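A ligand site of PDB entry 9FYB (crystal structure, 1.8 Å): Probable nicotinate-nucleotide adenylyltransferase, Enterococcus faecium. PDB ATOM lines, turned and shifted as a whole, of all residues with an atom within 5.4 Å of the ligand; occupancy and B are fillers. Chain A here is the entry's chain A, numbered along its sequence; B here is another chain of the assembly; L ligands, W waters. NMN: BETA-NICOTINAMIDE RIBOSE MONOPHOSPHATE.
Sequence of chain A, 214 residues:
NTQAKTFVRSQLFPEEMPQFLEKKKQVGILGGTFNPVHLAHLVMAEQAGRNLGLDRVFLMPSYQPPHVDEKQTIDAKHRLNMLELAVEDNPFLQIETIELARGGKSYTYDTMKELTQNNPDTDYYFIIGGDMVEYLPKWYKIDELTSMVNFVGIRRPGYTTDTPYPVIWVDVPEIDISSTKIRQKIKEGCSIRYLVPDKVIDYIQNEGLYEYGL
OH of Tyr 124 is in hydrogen-bond range of O2R of the ligand (2.4 Å). An oxygen (O3R) of the ligand lies within hydrogen-bond range of the side-chain carboxylate (OE1) of Glu 96 of chain A. An oxygen (O4R) of the ligand sits at hydrogen-bond distance from the side-chain amide nitrogen (ND2) of Asn 119 of chain B (2.5 Å). The guanidinium group of Arg 56 is in hydrogen-bond range of an oxygen (O7) of the ligand (2.8 Å). O2P of the ligand lies within hydrogen-bond range of ND2 of Asn 118 of chain B (2.8 Å).
The side-chain hydroxyl of Tyr 124 sits at hydrogen-bond distance from the backbone carbonyl oxygen of Leu 115 of chain A, at 3.2 Å. ND2 of Asn 119 of chain A lies within hydrogen-bond range of OH of Tyr 124 (2.9 Å). The side-chain carboxylate of Glu 96 of chain A is in hydrogen-bond range of the backbone NH of Ile 98 of chain A. O of Leu 115 of chain B lies close to OD1 of Asn 119 of chain B (2.9 Å). The side-chain carboxylate of Glu 96 of chain B is in hydrogen-bond range of the backbone NH of Ile 98 of chain B, 2.9 Å away. O of Leu 115 of chain A lies within hydrogen-bond range of ND2 of Asn 119 of chain A. The side-chain amino group (NZ) of Lys 25 of chain B sits at hydrogen-bond distance from the side-chain amide oxygen (OD1) of Asn 119 of chain A. The side-chain amino group (NZ) of Lys 25 of chain A lies within salt-bridge range of the side-chain carboxylate (OD2) of Asp 121 of chain A (3.2 Å).
OE2 of Glu 96 of chain B sits close to O1P of the ligand (3.2 Å). Lys 25 of chain A touches the ligand (CB to C4, 3.8 Å). CG2 of Val 27 touches C4 of the ligand, 3.7 Å away. CE2 of Phe 58 touches C5R of the ligand (3.5 Å). Ile 95 touches the ligand (O to O2P, 3.6 Å). Leu 115 of chain A touches the ligand. Asn 119 of chain A touches the ligand. Thr 122 touches the ligand. Ile 98 of chain B touches the ligand (CB to O1P, 3.9 Å). CD2 of Leu 115 of chain B touches O1P of the ligand, at 3.2 Å. Pro 120 of chain B touches the ligand. Asp 121 of chain B touches the ligand (OD2 to C4, 3.5 Å). Within 4 Å of the ligand: Lys 25 of chain A, Val 27, Arg 56, Phe 58, Ile 95, Glu 96 of chain A, Leu 115 of chain A, Asn 119 of chain A, Thr 122, Tyr 124, Glu 96 of chain B, Ile 98 of chain B, Leu 115 of chain B, Asn 118 of chain B, Asn 119 of chain B, Pro 120 of chain B and Asp 121 of chain B. The nearest printed residue that does not touch the ligand is Lys 25 of chain B (4.2 Å).
Water W1 bridges O3P of the ligand (2.4 Å) and OE2 of Glu 96 of chain A (3.4 Å).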
ATOM      1  N   LYS A  25       3.333  -3.085  22.938  1.00  0.00           N
ATOM      2  CA  LYS A  25       2.363  -3.352  21.892  1.00  0.00           C
ATOM      3  C   LYS A  25       1.552  -4.591  22.274  1.00  0.00           C
ATOM      4  O   LYS A  25       2.041  -5.473  22.982  1.00  0.00           O
ATOM      5  CB  LYS A  25       3.064  -3.553  20.558  1.00  0.00           C
ATOM      6  CG  LYS A  25       3.617  -2.235  20.013  1.00  0.00           C
ATOM      7  CD  LYS A  25       5.057  -2.094  20.440  1.00  0.00           C
ATOM      8  CE  LYS A  25       5.677  -0.782  19.966  1.00  0.00           C
ATOM      9  NZ  LYS A  25       6.604  -0.239  20.993  1.00  0.00           N
ATOM     10  N   VAL A  27      -0.485  -7.643  20.775  1.00  0.00           N
ATOM     11  CA  VAL A  27      -0.511  -8.305  19.486  1.00  0.00           C
ATOM     12  C   VAL A  27      -1.124  -9.679  19.614  1.00  0.00           C
ATOM     13  O   VAL A  27      -0.690 -10.493  20.450  1.00  0.00           O
ATOM     14  CB  VAL A  27       0.912  -8.404  18.892  1.00  0.00           C
ATOM     15  CG1 VAL A  27       0.900  -9.183  17.601  1.00  0.00           C
ATOM     16  CG2 VAL A  27       1.477  -6.990  18.661  1.00  0.00           C
ATOM     17  N   ASP A  55      -3.577  -4.157  19.111  1.00  0.00           N
ATOM     18  CA  ASP A  55      -2.982  -3.332  18.048  1.00  0.00           C
ATOM     19  C   ASP A  55      -2.986  -4.038  16.690  1.00  0.00           C
ATOM     20  O   ASP A  55      -3.002  -3.373  15.646  1.00  0.00           O
ATOM     21  CB  ASP A  55      -1.527  -2.980  18.371  1.00  0.00           C
ATOM     22  CG  ASP A  55      -1.385  -2.063  19.598  1.00  0.00           C
ATOM     23  OD1 ASP A  55      -2.252  -1.185  19.804  1.00  0.00           O
ATOM     24  OD2 ASP A  55      -0.400  -2.216  20.343  1.00  0.00           O
ATOM     25  N   ARG A  56      -2.966  -5.364  16.677  1.00  0.00           N
ATOM     26  CA  ARG A  56      -2.768  -6.121  15.443  1.00  0.00           C
ATOM     27  C   ARG A  56      -3.077  -7.562  15.760  1.00  0.00           C
ATOM     28  O   ARG A  56      -2.940  -7.963  16.908  1.00  0.00           O
ATOM     29  CB  ARG A  56      -1.317  -6.041  14.932  1.00  0.00           C
ATOM     30  CG  ARG A  56      -1.205  -5.883  13.420  1.00  0.00           C
ATOM     31  CD  ARG A  56      -1.607  -4.479  13.023  1.00  0.00           C
ATOM     32  NE  ARG A  56      -1.384  -4.168  11.622  1.00  0.00           N
ATOM     33  CZ  ARG A  56      -0.197  -4.017  11.035  1.00  0.00           C
ATOM     34  NH1 ARG A  56       0.931  -4.137  11.719  1.00  0.00           N
ATOM     35  NH2 ARG A  56      -0.155  -3.737   9.732  1.00  0.00           N
ATOM     36  N   PHE A  58      -1.923 -11.333  13.955  1.00  0.00           N
ATOM     37  CA  PHE A  58      -1.193 -12.068  12.951  1.00  0.00           C
ATOM     38  C   PHE A  58      -1.761 -13.470  12.839  1.00  0.00           C
ATOM     39  O   PHE A  58      -1.859 -14.164  13.854  1.00  0.00           O
ATOM     40  CB  PHE A  58       0.287 -12.159  13.321  1.00  0.00           C
ATOM     41  CG  PHE A  58       1.067 -10.874  13.104  1.00  0.00           C
ATOM     42  CD1 PHE A  58       0.960  -9.824  14.017  1.00  0.00           C
ATOM     43  CD2 PHE A  58       1.924 -10.720  12.011  1.00  0.00           C
ATOM     44  CE1 PHE A  58       1.681  -8.645  13.842  1.00  0.00           C
ATOM     45  CE2 PHE A  58       2.638  -9.529  11.831  1.00  0.00           C
ATOM     46  CZ  PHE A  58       2.499  -8.501  12.758  1.00  0.00           C
ATOM     47  N   ILE A  95       0.352 -11.523   8.510  1.00  0.00           N
ATOM     48  CA  ILE A  95       0.745 -12.917   8.451  1.00  0.00           C
ATOM     49  C   ILE A  95       2.067 -13.064   9.187  1.00  0.00           C
ATOM     50  O   ILE A  95       3.004 -12.303   8.933  1.00  0.00           O
ATOM     51  CB  ILE A  95       0.870 -13.396   6.988  1.00  0.00           C
ATOM     52  CG1 ILE A  95      -0.459 -13.230   6.225  1.00  0.00           C
ATOM     53  CG2 ILE A  95       1.338 -14.840   6.915  1.00  0.00           C
ATOM     54  CD1 ILE A  95      -1.688 -13.709   7.005  1.00  0.00           C
ATOM     55  N   GLU A  96       2.137 -14.023  10.115  1.00  0.00           N
ATOM     56  CA  GLU A  96       3.393 -14.338  10.782  1.00  0.00           C
ATOM     57  C   GLU A  96       3.945 -15.634  10.197  1.00  0.00           C
ATOM     58  O   GLU A  96       3.337 -16.696  10.360  1.00  0.00           O
ATOM     59  CB  GLU A  96       3.189 -14.455  12.294  1.00  0.00           C
ATOM     60  CG  GLU A  96       4.427 -15.027  13.028  1.00  0.00           C
ATOM     61  CD  GLU A  96       5.671 -14.172  12.844  1.00  0.00           C
ATOM     62  OE1 GLU A  96       5.634 -12.977  13.196  1.00  0.00           O
ATOM     63  OE2 GLU A  96       6.668 -14.703  12.323  1.00  0.00           O
ATOM     64  N   THR A  97       5.092 -15.558   9.521  1.00  0.00           N
ATOM     65  CA  THR A  97       5.621 -16.692   8.772  1.00  0.00           C
ATOM     66  C   THR A  97       6.788 -17.419   9.456  1.00  0.00           C
ATOM     67  O   THR A  97       7.450 -18.221   8.812  1.00  0.00           O
ATOM     68  CB  THR A  97       6.027 -16.259   7.353  1.00  0.00           C
ATOM     69  OG1 THR A  97       7.000 -15.201   7.414  1.00  0.00           O
ATOM     70  CG2 THR A  97       4.832 -15.773   6.588  1.00  0.00           C
ATOM     71  N   ILE A  98       7.012 -17.222  10.767  1.00  0.00           N
ATOM     72  CA  ILE A  98       8.199 -17.828  11.378  1.00  0.00           C
ATOM     73  C   ILE A  98       8.126 -19.352  11.347  1.00  0.00           C
ATOM     74  O   ILE A  98       9.140 -20.034  11.159  1.00  0.00           O
ATOM     75  CB  ILE A  98       8.411 -17.314  12.816  1.00  0.00           C
ATOM     76  CG1 ILE A  98       9.742 -17.823  13.388  1.00  0.00           C
ATOM     77  CG2 ILE A  98       7.244 -17.711  13.714  1.00  0.00           C
ATOM     78  CD1 ILE A  98      10.111 -17.189  14.742  1.00  0.00           C
ATOM     79  N   LEU A 115       9.605 -15.507  19.303  1.00  0.00           N
ATOM     80  CA  LEU A 115       8.938 -14.225  19.034  1.00  0.00           C
ATOM     81  C   LEU A 115       9.036 -13.263  20.201  1.00  0.00           C
ATOM     82  O   LEU A 115       9.192 -12.054  19.991  1.00  0.00           O
ATOM     83  CB  LEU A 115       7.467 -14.407  18.636  1.00  0.00           C
ATOM     84  CG  LEU A 115       7.150 -15.081  17.300  1.00  0.00           C
ATOM     85  CD1 LEU A 115       5.646 -15.316  17.185  1.00  0.00           C
ATOM     86  CD2 LEU A 115       7.654 -14.247  16.144  1.00  0.00           C
ATOM     87  N   ASN A 119      10.830  -9.784  20.044  1.00  0.00           N
ATOM     88  CA  ASN A 119       9.994  -8.600  20.276  1.00  0.00           C
ATOM     89  C   ASN A 119       9.718  -8.487  21.765  1.00  0.00           C
ATOM     90  O   ASN A 119       8.599  -8.728  22.234  1.00  0.00           O
ATOM     91  CB  ASN A 119       8.684  -8.688  19.496  1.00  0.00           C
ATOM     92  CG  ASN A 119       8.914  -8.892  18.028  1.00  0.00           C
ATOM     93  OD1 ASN A 119       9.267  -7.948  17.338  1.00  0.00           O
ATOM     94  ND2 ASN A 119       8.758 -10.131  17.543  1.00  0.00           N
ATOM     95  N   ASP A 121       9.300  -6.026  23.567  1.00  0.00           N
ATOM     96  CA  ASP A 121       8.386  -4.940  23.865  1.00  0.00           C
ATOM     97  C   ASP A 121       6.938  -5.290  23.577  1.00  0.00           C
ATOM     98  O   ASP A 121       6.104  -4.374  23.470  1.00  0.00           O
ATOM     99  CB  ASP A 121       8.762  -3.720  23.028  1.00  0.00           C
ATOM    100  CG  ASP A 121       8.562  -3.965  21.540  1.00  0.00           C
ATOM    101  OD1 ASP A 121       8.984  -5.047  21.033  1.00  0.00           O
ATOM    102  OD2 ASP A 121       8.004  -3.073  20.868  1.00  0.00           O
ATOM    103  N   THR A 122       6.623  -6.565  23.364  1.00  0.00           N
ATOM    104  CA  THR A 122       5.300  -6.945  22.880  1.00  0.00           C
ATOM    105  C   THR A 122       4.652  -7.923  23.855  1.00  0.00           C
ATOM    106  O   THR A 122       5.265  -8.910  24.261  1.00  0.00           O
ATOM    107  CB  THR A 122       5.384  -7.602  21.492  1.00  0.00           C
ATOM    108  OG1 THR A 122       5.948  -6.661  20.569  1.00  0.00           O
ATOM    109  CG2 THR A 122       3.976  -8.033  21.029  1.00  0.00           C
ATOM    110  N   TYR A 124       1.920 -10.686  23.937  1.00  0.00           N
ATOM    111  CA  TYR A 124       1.299 -11.562  22.938  1.00  0.00           C
ATOM    112  C   TYR A 124      -0.002 -12.170  23.453  1.00  0.00           C
ATOM    113  O   TYR A 124      -0.090 -12.539  24.624  1.00  0.00           O
ATOM    114  CB  TYR A 124       2.264 -12.655  22.497  1.00  0.00           C
ATOM    115  CG  TYR A 124       3.340 -12.202  21.551  1.00  0.00           C
ATOM    116  CD1 TYR A 124       3.058 -11.945  20.222  1.00  0.00           C
ATOM    117  CD2 TYR A 124       4.645 -12.051  21.987  1.00  0.00           C
ATOM    118  CE1 TYR A 124       4.050 -11.537  19.350  1.00  0.00           C
ATOM    119  CE2 TYR A 124       5.644 -11.633  21.127  1.00  0.00           C
ATOM    120  CZ  TYR A 124       5.347 -11.382  19.804  1.00  0.00           C
ATOM    121  OH  TYR A 124       6.348 -10.983  18.959  1.00  0.00           O
ATOM    122  N   LYS B  25      11.070   1.445  17.671  1.00  0.00           N
ATOM    123  CA  LYS B  25      12.175   0.502  17.804  1.00  0.00           C
ATOM    124  C   LYS B  25      13.211   0.773  16.726  1.00  0.00           C
ATOM    125  O   LYS B  25      12.865   1.012  15.562  1.00  0.00           O
ATOM    126  CB  LYS B  25      11.610  -0.910  17.706  1.00  0.00           C
ATOM    127  CG  LYS B  25      11.105  -1.413  19.045  1.00  0.00           C
ATOM    128  CD  LYS B  25      10.385  -2.766  18.972  1.00  0.00           C
ATOM    129  CE  LYS B  25       9.940  -3.182  17.574  1.00  0.00           C
ATOM    130  NZ  LYS B  25       9.188  -4.483  17.620  1.00  0.00           N
ATOM    131  N   GLU B  96      16.021 -12.974  11.387  1.00  0.00           N
ATOM    132  CA  GLU B  96      14.812 -12.582  10.668  1.00  0.00           C
ATOM    133  C   GLU B  96      14.596 -13.557   9.511  1.00  0.00           C
ATOM    134  O   GLU B  96      15.377 -13.566   8.553  1.00  0.00           O
ATOM    135  CB  GLU B  96      14.927 -11.141  10.163  1.00  0.00           C
ATOM    136  CG  GLU B  96      13.840 -10.755   9.187  1.00  0.00           C
ATOM    137  CD  GLU B  96      12.433 -10.960   9.774  1.00  0.00           C
ATOM    138  OE1 GLU B  96      12.094 -10.253  10.754  1.00  0.00           O
ATOM    139  OE2 GLU B  96      11.703 -11.827   9.256  1.00  0.00           O
ATOM    140  N   ILE B  98      11.941 -13.995   7.322  1.00  0.00           N
ATOM    141  CA  ILE B  98      10.832 -13.776   6.382  1.00  0.00           C
ATOM    142  C   ILE B  98      11.226 -14.175   4.966  1.00  0.00           C
ATOM    143  O   ILE B  98      10.386 -14.677   4.186  1.00  0.00           O
ATOM    144  CB  ILE B  98      10.340 -12.315   6.464  1.00  0.00           C
ATOM    145  CG1 ILE B  98       9.102 -12.111   5.586  1.00  0.00           C
ATOM    146  CG2 ILE B  98      11.444 -11.326   6.098  1.00  0.00           C
ATOM    147  CD1 ILE B  98       8.628 -10.647   5.554  1.00  0.00           C
ATOM    148  N   LEU B 115       8.033  -6.089   5.907  1.00  0.00           N
ATOM    149  CA  LEU B 115       8.522  -5.894   7.268  1.00  0.00           C
ATOM    150  C   LEU B 115       8.037  -4.570   7.864  1.00  0.00           C
ATOM    151  O   LEU B 115       7.657  -4.512   9.038  1.00  0.00           O
ATOM    152  CB  LEU B 115      10.050  -5.933   7.296  1.00  0.00           C
ATOM    153  CG  LEU B 115      10.763  -7.280   7.279  1.00  0.00           C
ATOM    154  CD1 LEU B 115      12.247  -7.046   7.616  1.00  0.00           C
ATOM    155  CD2 LEU B 115      10.110  -8.259   8.241  1.00  0.00           C
ATOM    156  N   GLN B 117       5.345  -3.032   6.972  1.00  0.00           N
ATOM    157  CA  GLN B 117       3.903  -3.159   7.189  1.00  0.00           C
ATOM    158  C   GLN B 117       3.615  -3.957   8.446  1.00  0.00           C
ATOM    159  O   GLN B 117       2.708  -3.612   9.218  1.00  0.00           O
ATOM    160  CB  GLN B 117       3.189  -3.819   6.009  1.00  0.00           C
ATOM    161  CG  GLN B 117       3.185  -3.041   4.727  1.00  0.00           C
ATOM    162  CD  GLN B 117       2.643  -3.860   3.572  1.00  0.00           C
ATOM    163  OE1 GLN B 117       2.822  -5.083   3.513  1.00  0.00           O
ATOM    164  NE2 GLN B 117       2.011  -3.180   2.629  1.00  0.00           N
ATOM    165  N   ASN B 118       4.310  -5.080   8.638  1.00  0.00           N
ATOM    166  CA  ASN B 118       4.144  -5.838   9.859  1.00  0.00           C
ATOM    167  C   ASN B 118       4.565  -5.045  11.081  1.00  0.00           C
ATOM    168  O   ASN B 118       4.021  -5.260  12.169  1.00  0.00           O
ATOM    169  CB  ASN B 118       4.964  -7.132   9.797  1.00  0.00           C
ATOM    170  CG  ASN B 118       4.346  -8.182   8.901  1.00  0.00           C
ATOM    171  OD1 ASN B 118       3.337  -7.952   8.241  1.00  0.00           O
ATOM    172  ND2 ASN B 118       4.980  -9.350   8.859  1.00  0.00           N
ATOM    173  N   ASN B 119       5.529  -4.134  10.927  1.00  0.00           N
ATOM    174  CA  ASN B 119       6.195  -3.518  12.075  1.00  0.00           C
ATOM    175  C   ASN B 119       6.206  -2.000  11.940  1.00  0.00           C
ATOM    176  O   ASN B 119       7.262  -1.381  11.840  1.00  0.00           O
ATOM    177  CB  ASN B 119       7.609  -4.063  12.238  1.00  0.00           C
ATOM    178  CG  ASN B 119       7.639  -5.581  12.280  1.00  0.00           C
ATOM    179  OD1 ASN B 119       8.101  -6.238  11.340  1.00  0.00           O
ATOM    180  ND2 ASN B 119       7.158  -6.140  13.366  1.00  0.00           N
ATOM    181  N   PRO B 120       5.025  -1.370  11.984  1.00  0.00           N
ATOM    182  CA  PRO B 120       4.960   0.095  11.775  1.00  0.00           C
ATOM    183  C   PRO B 120       5.648   0.884  12.863  1.00  0.00           C
ATOM    184  O   PRO B 120       5.948   2.074  12.671  1.00  0.00           O
ATOM    185  CB  PRO B 120       3.450   0.375  11.727  1.00  0.00           C
ATOM    186  CG  PRO B 120       2.835  -0.699  12.559  1.00  0.00           C
ATOM    187  CD  PRO B 120       3.717  -1.931  12.356  1.00  0.00           C
ATOM    188  N   ASP B 121       5.896   0.283  14.008  1.00  0.00           N
ATOM    189  CA  ASP B 121       6.623   0.919  15.100  1.00  0.00           C
ATOM    190  C   ASP B 121       8.142   0.878  14.916  1.00  0.00           C
ATOM    191  O   ASP B 121       8.867   1.356  15.798  1.00  0.00           O
ATOM    192  CB  ASP B 121       6.252   0.207  16.404  1.00  0.00           C
ATOM    193  CG  ASP B 121       6.339  -1.322  16.284  1.00  0.00           C
ATOM    194  OD1 ASP B 121       6.703  -1.831  15.197  1.00  0.00           O
ATOM    195  OD2 ASP B 121       6.069  -2.021  17.286  1.00  0.00           O
HETATM  196  O3P NMN L   1       8.158 -12.190  11.620  1.00  0.00           O
HETATM  197  P   NMN L   1       7.646 -11.113  10.687  1.00  0.00           P
HETATM  198  O1P NMN L   1       8.688 -10.712   9.672  1.00  0.00           O
HETATM  199  O2P NMN L   1       6.322 -11.479  10.057  1.00  0.00           O
HETATM  200  O5R NMN L   1       7.393  -9.803  11.608  1.00  0.00           O
HETATM  201  C5R NMN L   1       6.101  -9.623  12.260  1.00  0.00           C
HETATM  202  C4R NMN L   1       6.276  -9.507  13.754  1.00  0.00           C
HETATM  203  O4R NMN L   1       6.011  -8.148  14.189  1.00  0.00           O
HETATM  204  C3R NMN L   1       5.331 -10.348  14.625  1.00  0.00           C
HETATM  205  O3R NMN L   1       5.984 -11.508  15.127  1.00  0.00           O
HETATM  206  C2R NMN L   1       4.926  -9.440  15.788  1.00  0.00           C
HETATM  207  O2R NMN L   1       5.266  -9.965  17.054  1.00  0.00           O
HETATM  208  C1R NMN L   1       5.811  -8.218  15.583  1.00  0.00           C
HETATM  209  N1  NMN L   1       5.165  -6.994  16.079  1.00  0.00           N
HETATM  210  C2  NMN L   1       4.171  -6.382  15.357  1.00  0.00           C
HETATM  211  C3  NMN L   1       3.562  -5.238  15.864  1.00  0.00           C
HETATM  212  C7  NMN L   1       2.489  -4.555  15.073  1.00  0.00           C
HETATM  213  O7  NMN L   1       1.974  -5.121  14.107  1.00  0.00           O
HETATM  214  N7  NMN L   1       2.100  -3.347  15.479  1.00  0.00           N
HETATM  215  C4  NMN L   1       3.940  -4.734  17.095  1.00  0.00           C
HETATM  216  C5  NMN L   1       4.925  -5.384  17.822  1.00  0.00           C
HETATM  217  C6  NMN L   1       5.526  -6.506  17.318  1.00  0.00           C
HETATM  218  O   HOH W   1       9.660 -13.347  13.140  1.00  0.00           O
